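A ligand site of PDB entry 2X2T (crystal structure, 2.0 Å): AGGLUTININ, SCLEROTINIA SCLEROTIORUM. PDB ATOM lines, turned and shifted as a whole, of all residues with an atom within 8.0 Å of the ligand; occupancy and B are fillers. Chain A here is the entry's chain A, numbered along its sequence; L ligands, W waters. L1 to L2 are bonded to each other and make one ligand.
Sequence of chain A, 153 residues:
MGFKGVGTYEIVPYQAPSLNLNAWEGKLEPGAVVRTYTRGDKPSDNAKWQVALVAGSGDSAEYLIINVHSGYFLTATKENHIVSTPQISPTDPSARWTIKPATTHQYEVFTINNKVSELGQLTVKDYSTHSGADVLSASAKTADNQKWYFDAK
The side-chain amino group (NZ) of Lys 27 lies within salt-bridge range of the side-chain carboxylate (OE1) of Glu 25. The side-chain amide nitrogen of Asn 46 sits at hydrogen-bond distance from the side-chain amide oxygen of Asn 22, at 3.3 Å. The backbone NH of Asn 22 is in hydrogen-bond range of the backbone carbonyl oxygen of Arg 35. The side-chain amide nitrogen (ND2) of Asn 46 is in hydrogen-bond range of the backbone carbonyl oxygen (O) of Ala 23 (3.0 Å). OG of Ser 44 is in hydrogen-bond range of OD1 of Asn 46 (2.6 Å). N of Trp 24 lies within hydrogen-bond range of O of Val 33 (2.9 Å). O of Tyr 37 is in hydrogen-bond range of N of Asn 20, at 2.9 Å.
An oxygen (O3) of LG2 L2 is in hydrogen-bond range of the backbone NH (N) of Glu 25, 2.8 Å away. The backbone carbonyl oxygen (O) of Glu 25 lies within hydrogen-bond range of an oxygen (O3) of LIG L1, 2.7 Å away. The side-chain carboxylate of Glu 25 sits at hydrogen-bond distance from an oxygen (O5) of LIG L1, 2.9 Å away. OD1 of Asn 22 sits at hydrogen-bond distance from O3 of LG2 L2 (2.8 Å). ND2 of Asn 46 sits at hydrogen-bond distance from O2 of LG2 L2 (3.0 Å).
Water W6 bridges an oxygen (O2) of LG2 L2 (2.7 Å) and the side-chain hydroxyl (OG) of Ser 44 (3.1 Å). Water W7 lies within hydrogen-bond range of OD1 of Asn 46 (2.7 Å) and O1 of LG2 L2 (2.8 Å). Water W5 lies within hydrogen-bond range of the side-chain carboxylate (OE1) of Glu 25, the side-chain amino group (NZ) of Lys 27 and an oxygen (O5) of LIG L1.
Residues that only touch the ligand: Ala 23, Trp 24 and Tyr 37. Hydrophobic or aromatic side chains that line the ligand: Trp 24 and Tyr 37. Six residues have an atom within 4 Å of the ligand: Asn 22, Ala 23, Trp 24, Glu 25, Tyr 37 and Asn 46. The nearest printed residue that does not touch the ligand is Lys 27 (4.2 Å).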
ATOM      1  N   ASN A  20      -3.260 -24.300 -25.767  1.00  0.00           N
ATOM      2  CA  ASN A  20      -3.825 -23.013 -25.391  1.00  0.00           C
ATOM      3  C   ASN A  20      -2.821 -22.126 -24.660  1.00  0.00           C
ATOM      4  O   ASN A  20      -1.688 -22.526 -24.407  1.00  0.00           O
ATOM      5  CB  ASN A  20      -5.116 -23.213 -24.613  1.00  0.00           C
ATOM      6  CG  ASN A  20      -4.910 -23.912 -23.271  1.00  0.00           C
ATOM      7  OD1 ASN A  20      -3.814 -23.900 -22.702  1.00  0.00           O
ATOM      8  ND2 ASN A  20      -5.975 -24.499 -22.745  1.00  0.00           N
ATOM      9  N   ASN A  22      -1.299 -20.477 -21.553  1.00  0.00           N
ATOM     10  CA  ASN A  22      -1.107 -21.093 -20.220  1.00  0.00           C
ATOM     11  C   ASN A  22      -0.171 -20.248 -19.331  1.00  0.00           C
ATOM     12  O   ASN A  22       0.942 -19.972 -19.725  1.00  0.00           O
ATOM     13  CB  ASN A  22      -0.506 -22.499 -20.422  1.00  0.00           C
ATOM     14  CG  ASN A  22      -0.324 -23.288 -19.118  1.00  0.00           C
ATOM     15  OD1 ASN A  22       0.524 -22.951 -18.298  1.00  0.00           O
ATOM     16  ND2 ASN A  22      -1.113 -24.352 -18.939  1.00  0.00           N
ATOM     17  N   ALA A  23      -0.645 -19.852 -18.146  1.00  0.00           N
ATOM     18  CA  ALA A  23       0.154 -19.181 -17.139  1.00  0.00           C
ATOM     19  C   ALA A  23       0.992 -20.267 -16.481  1.00  0.00           C
ATOM     20  O   ALA A  23       0.472 -21.053 -15.696  1.00  0.00           O
ATOM     21  CB  ALA A  23      -0.724 -18.488 -16.084  1.00  0.00           C
ATOM     22  N   TRP A  24       2.267 -20.287 -16.821  1.00  0.00           N
ATOM     23  CA  TRP A  24       3.179 -21.412 -16.541  1.00  0.00           C
ATOM     24  C   TRP A  24       3.309 -21.671 -15.049  1.00  0.00           C
ATOM     25  O   TRP A  24       3.565 -20.750 -14.273  1.00  0.00           O
ATOM     26  CB  TRP A  24       4.562 -21.098 -17.114  1.00  0.00           C
ATOM     27  CG  TRP A  24       5.446 -22.282 -17.417  1.00  0.00           C
ATOM     28  CD1 TRP A  24       6.625 -22.606 -16.807  1.00  0.00           C
ATOM     29  CD2 TRP A  24       5.240 -23.258 -18.437  1.00  0.00           C
ATOM     30  NE1 TRP A  24       7.164 -23.727 -17.390  1.00  0.00           N
ATOM     31  CE2 TRP A  24       6.331 -24.146 -18.393  1.00  0.00           C
ATOM     32  CE3 TRP A  24       4.238 -23.461 -19.382  1.00  0.00           C
ATOM     33  CZ2 TRP A  24       6.442 -25.239 -19.262  1.00  0.00           C
ATOM     34  CZ3 TRP A  24       4.355 -24.544 -20.258  1.00  0.00           C
ATOM     35  CH2 TRP A  24       5.457 -25.415 -20.191  1.00  0.00           C
ATOM     36  N   GLU A  25       3.094 -22.936 -14.666  1.00  0.00           N
ATOM     37  CA  GLU A  25       3.129 -23.431 -13.287  1.00  0.00           C
ATOM     38  C   GLU A  25       1.788 -23.291 -12.548  1.00  0.00           C
ATOM     39  O   GLU A  25       1.562 -24.002 -11.592  1.00  0.00           O
ATOM     40  CB  GLU A  25       4.260 -22.849 -12.426  1.00  0.00           C
ATOM     41  CG  GLU A  25       5.641 -22.975 -13.035  1.00  0.00           C
ATOM     42  CD  GLU A  25       6.757 -22.716 -12.025  1.00  0.00           C
ATOM     43  OE1 GLU A  25       6.871 -23.453 -11.031  1.00  0.00           O
ATOM     44  OE2 GLU A  25       7.535 -21.785 -12.254  1.00  0.00           O
ATOM     45  N   GLY A  26       0.922 -22.378 -12.995  1.00  0.00           N
ATOM     46  CA  GLY A  26      -0.444 -22.288 -12.464  1.00  0.00           C
ATOM     47  C   GLY A  26      -0.499 -22.023 -10.979  1.00  0.00           C
ATOM     48  O   GLY A  26      -1.346 -22.587 -10.253  1.00  0.00           O
ATOM     49  N   LYS A  27       0.429 -21.192 -10.509  1.00  0.00           N
ATOM     50  CA  LYS A  27       0.534 -20.795  -9.105  1.00  0.00           C
ATOM     51  C   LYS A  27      -0.173 -19.474  -8.832  1.00  0.00           C
ATOM     52  O   LYS A  27      -0.539 -18.754  -9.760  1.00  0.00           O
ATOM     53  CB  LYS A  27       1.994 -20.665  -8.716  1.00  0.00           C
ATOM     54  CG  LYS A  27       2.751 -21.967  -8.694  1.00  0.00           C
ATOM     55  CD  LYS A  27       4.224 -21.686  -8.623  1.00  0.00           C
ATOM     56  CE  LYS A  27       4.989 -22.881  -8.148  1.00  0.00           C
ATOM     57  NZ  LYS A  27       6.435 -22.523  -8.015  1.00  0.00           N
ATOM     58  N   VAL A  33       5.263 -16.361 -16.184  1.00  0.00           N
ATOM     59  CA  VAL A  33       5.362 -16.195 -17.645  1.00  0.00           C
ATOM     60  C   VAL A  33       4.280 -17.036 -18.332  1.00  0.00           C
ATOM     61  O   VAL A  33       3.669 -17.941 -17.715  1.00  0.00           O
ATOM     62  CB  VAL A  33       6.802 -16.464 -18.206  1.00  0.00           C
ATOM     63  CG1 VAL A  33       7.808 -15.577 -17.503  1.00  0.00           C
ATOM     64  CG2 VAL A  33       7.224 -17.927 -18.039  1.00  0.00           C
ATOM     65  N   ARG A  35       3.050 -19.348 -21.743  1.00  0.00           N
ATOM     66  CA  ARG A  35       3.477 -20.204 -22.824  1.00  0.00           C
ATOM     67  C   ARG A  35       2.265 -20.914 -23.442  1.00  0.00           C
ATOM     68  O   ARG A  35       1.188 -20.922 -22.868  1.00  0.00           O
ATOM     69  CB  ARG A  35       4.483 -21.256 -22.345  1.00  0.00           C
ATOM     70  CG  ARG A  35       5.755 -20.660 -21.764  1.00  0.00           C
ATOM     71  CD  ARG A  35       6.921 -21.641 -21.678  1.00  0.00           C
ATOM     72  NE  ARG A  35       8.164 -20.921 -21.419  1.00  0.00           N
ATOM     73  CZ  ARG A  35       8.696 -20.665 -20.218  1.00  0.00           C
ATOM     74  NH1 ARG A  35       9.819 -19.975 -20.138  1.00  0.00           N
ATOM     75  NH2 ARG A  35       8.119 -21.083 -19.104  1.00  0.00           N
ATOM     76  N   THR A  36       2.459 -21.527 -24.604  1.00  0.00           N
ATOM     77  CA  THR A  36       1.515 -22.507 -25.082  1.00  0.00           C
ATOM     78  C   THR A  36       1.690 -23.809 -24.281  1.00  0.00           C
ATOM     79  O   THR A  36       2.804 -24.144 -23.803  1.00  0.00           O
ATOM     80  CB  THR A  36       1.676 -22.767 -26.609  1.00  0.00           C
ATOM     81  OG1 THR A  36       2.896 -23.467 -26.845  1.00  0.00           O
ATOM     82  CG2 THR A  36       1.647 -21.453 -27.421  1.00  0.00           C
ATOM     83  N   TYR A  37       0.582 -24.553 -24.112  1.00  0.00           N
ATOM     84  CA  TYR A  37       0.609 -25.849 -23.421  1.00  0.00           C
ATOM     85  C   TYR A  37      -0.548 -26.668 -23.893  1.00  0.00           C
ATOM     86  O   TYR A  37      -1.607 -26.123 -24.276  1.00  0.00           O
ATOM     87  CB  TYR A  37       0.498 -25.650 -21.912  1.00  0.00           C
ATOM     88  CG  TYR A  37       0.916 -26.803 -21.022  1.00  0.00           C
ATOM     89  CD1 TYR A  37       2.251 -27.206 -20.953  1.00  0.00           C
ATOM     90  CD2 TYR A  37      -0.012 -27.459 -20.188  1.00  0.00           C
ATOM     91  CE1 TYR A  37       2.665 -28.214 -20.078  1.00  0.00           C
ATOM     92  CE2 TYR A  37       0.411 -28.486 -19.291  1.00  0.00           C
ATOM     93  CZ  TYR A  37       1.757 -28.843 -19.257  1.00  0.00           C
ATOM     94  OH  TYR A  37       2.236 -29.838 -18.426  1.00  0.00           O
ATOM     95  N   THR A  38      -0.374 -27.979 -23.822  1.00  0.00           N
ATOM     96  CA  THR A  38      -1.444 -28.927 -24.111  1.00  0.00           C
ATOM     97  C   THR A  38      -2.779 -28.532 -23.450  1.00  0.00           C
ATOM     98  O   THR A  38      -2.839 -28.266 -22.235  1.00  0.00           O
ATOM     99  CB  THR A  38      -1.045 -30.331 -23.626  1.00  0.00           C
ATOM    100  OG1 THR A  38       0.207 -30.691 -24.223  1.00  0.00           O
ATOM    101  CG2 THR A  38      -2.127 -31.365 -23.994  1.00  0.00           C
ATOM    102  N   ARG A  39      -3.864 -28.498 -24.245  1.00  0.00           N
ATOM    103  CA  ARG A  39      -5.204 -28.161 -23.697  1.00  0.00           C
ATOM    104  C   ARG A  39      -5.711 -29.192 -22.669  1.00  0.00           C
ATOM    105  O   ARG A  39      -6.163 -28.821 -21.597  1.00  0.00           O
ATOM    106  CB  ARG A  39      -6.268 -27.989 -24.810  1.00  0.00           C
ATOM    107  CG  ARG A  39      -5.989 -26.773 -25.671  1.00  0.00           C
ATOM    108  CD  ARG A  39      -6.906 -26.675 -26.907  1.00  0.00           C
ATOM    109  NE  ARG A  39      -8.235 -26.176 -26.558  1.00  0.00           N
ATOM    110  CZ  ARG A  39      -9.168 -25.840 -27.441  1.00  0.00           C
ATOM    111  NH1 ARG A  39      -8.950 -25.950 -28.744  1.00  0.00           N
ATOM    112  NH2 ARG A  39     -10.347 -25.388 -27.003  1.00  0.00           N
ATOM    113  N   SER A  44      -7.402 -26.392 -17.642  1.00  0.00           N
ATOM    114  CA  SER A  44      -7.217 -26.029 -16.246  1.00  0.00           C
ATOM    115  C   SER A  44      -7.420 -24.520 -16.100  1.00  0.00           C
ATOM    116  O   SER A  44      -7.280 -23.780 -17.077  1.00  0.00           O
ATOM    117  CB  SER A  44      -5.827 -26.450 -15.819  1.00  0.00           C
ATOM    118  OG  SER A  44      -4.873 -25.836 -16.658  1.00  0.00           O
ATOM    119  N   ASP A  45      -7.716 -24.074 -14.882  1.00  0.00           N
ATOM    120  CA  ASP A  45      -8.015 -22.651 -14.643  1.00  0.00           C
ATOM    121  C   ASP A  45      -6.860 -21.696 -14.958  1.00  0.00           C
ATOM    122  O   ASP A  45      -7.078 -20.549 -15.322  1.00  0.00           O
ATOM    123  CB  ASP A  45      -8.485 -22.430 -13.196  1.00  0.00           C
ATOM    124  CG  ASP A  45      -9.939 -22.859 -12.960  1.00  0.00           C
ATOM    125  OD1 ASP A  45     -10.634 -23.260 -13.925  1.00  0.00           O
ATOM    126  OD2 ASP A  45     -10.383 -22.801 -11.809  1.00  0.00           O
ATOM    127  N   ASN A  46      -5.633 -22.160 -14.811  1.00  0.00           N
ATOM    128  CA  ASN A  46      -4.488 -21.337 -15.190  1.00  0.00           C
ATOM    129  C   ASN A  46      -4.369 -21.178 -16.720  1.00  0.00           C
ATOM    130  O   ASN A  46      -3.541 -20.399 -17.179  1.00  0.00           O
ATOM    131  CB  ASN A  46      -3.155 -21.875 -14.603  1.00  0.00           C
ATOM    132  CG  ASN A  46      -2.754 -23.235 -15.175  1.00  0.00           C
ATOM    133  OD1 ASN A  46      -3.543 -24.183 -15.146  1.00  0.00           O
ATOM    134  ND2 ASN A  46      -1.498 -23.341 -15.672  1.00  0.00           N
ATOM    135  N   ALA A  47      -5.187 -21.923 -17.480  1.00  0.00           N
ATOM    136  CA  ALA A  47      -5.210 -21.788 -18.943  1.00  0.00           C
ATOM    137  C   ALA A  47      -6.597 -21.344 -19.448  1.00  0.00           C
ATOM    138  O   ALA A  47      -6.975 -21.629 -20.588  1.00  0.00           O
ATOM    139  CB  ALA A  47      -4.753 -23.111 -19.617  1.00  0.00           C
ATOM    140  N   SER A 131       3.649 -27.974 -27.656  1.00  0.00           N
ATOM    141  CA  SER A 131       3.473 -27.515 -26.273  1.00  0.00           C
ATOM    142  C   SER A 131       4.784 -26.945 -25.704  1.00  0.00           C
ATOM    143  O   SER A 131       5.875 -27.421 -26.014  1.00  0.00           O
ATOM    144  CB  SER A 131       2.977 -28.685 -25.379  1.00  0.00           C
ATOM    145  OG  SER A 131       2.632 -28.247 -24.065  1.00  0.00           O
ATOM    146  N   GLY A 132       4.630 -25.912 -24.866  1.00  0.00           N
ATOM    147  CA  GLY A 132       5.747 -25.352 -24.112  1.00  0.00           C
ATOM    148  C   GLY A 132       6.520 -24.210 -24.738  1.00  0.00           C
ATOM    149  O   GLY A 132       7.602 -23.889 -24.263  1.00  0.00           O
HETATM  150  C1  LIG L   1       3.238 -29.139  -9.904  1.00  0.00           C
HETATM  151  C2  LIG L   1       2.224 -28.485 -10.843  1.00  0.00           C
HETATM  152  C3  LIG L   1       2.902 -27.744 -11.993  1.00  0.00           C
HETATM  153  C4  LIG L   1       3.973 -26.849 -11.449  1.00  0.00           C
HETATM  154  C5  LIG L   1       4.930 -27.673 -10.570  1.00  0.00           C
HETATM  155  C6  LIG L   1       6.036 -26.798 -10.016  1.00  0.00           C
HETATM  156  C7  LIG L   1       0.016 -29.432 -11.236  1.00  0.00           C
HETATM  157  C8  LIG L   1      -0.786 -30.532 -11.860  1.00  0.00           C
HETATM  158  N1  LIG L   1       1.319 -29.461 -11.404  1.00  0.00           N
HETATM  159  O1  LIG L   1       2.568 -29.712  -8.796  1.00  0.00           O
HETATM  160  O2  LIG L   1       1.904 -27.011 -12.684  1.00  0.00           O
HETATM  161  O3  LIG L   1       3.355 -25.839 -10.637  1.00  0.00           O
HETATM  162  O4  LIG L   1       4.168 -28.169  -9.469  1.00  0.00           O
HETATM  163  O5  LIG L   1       6.884 -26.332 -11.082  1.00  0.00           O
HETATM  164  O6  LIG L   1      -0.501 -28.550 -10.587  1.00  0.00           O
HETATM  165  C1  LG2 L   2       1.893 -27.213 -14.102  1.00  0.00           C
HETATM  166  C2  LG2 L   2       0.582 -26.694 -14.673  1.00  0.00           C
HETATM  167  C3  LG2 L   2       0.599 -26.694 -16.210  1.00  0.00           C
HETATM  168  C4  LG2 L   2       1.878 -26.037 -16.728  1.00  0.00           C
HETATM  169  C5  LG2 L   2       3.085 -26.705 -16.072  1.00  0.00           C
HETATM  170  C6  LG2 L   2       4.405 -26.155 -16.601  1.00  0.00           C
HETATM  171  O1  LG2 L   2      -0.539 -27.456 -14.172  1.00  0.00           O
HETATM  172  O2  LG2 L   2      -0.584 -26.046 -16.701  1.00  0.00           O
HETATM  173  O3  LG2 L   2       1.861 -24.618 -16.476  1.00  0.00           O
HETATM  174  O4  LG2 L   2       3.006 -26.490 -14.646  1.00  0.00           O
HETATM  175  O5  LG2 L   2       5.517 -26.936 -16.122  1.00  0.00           O
HETATM  176  O   HOH W   1       4.682 -31.001  -7.606  1.00  0.00           O
HETATM  177  O   HOH W   2       2.639 -25.593  -7.918  1.00  0.00           O
HETATM  178  O   HOH W   3       6.748 -26.183 -13.687  1.00  0.00           O
HETATM  179  O   HOH W   4       2.526 -32.371  -9.093  1.00  0.00           O
HETATM  180  O   HOH W   5       8.853 -24.004  -9.461  1.00  0.00           O
HETATM  181  O   HOH W   6      -2.575 -27.844 -17.233  1.00  0.00           O
HETATM  182  O   HOH W   7      -2.751 -26.017 -13.285  1.00  0.00           O
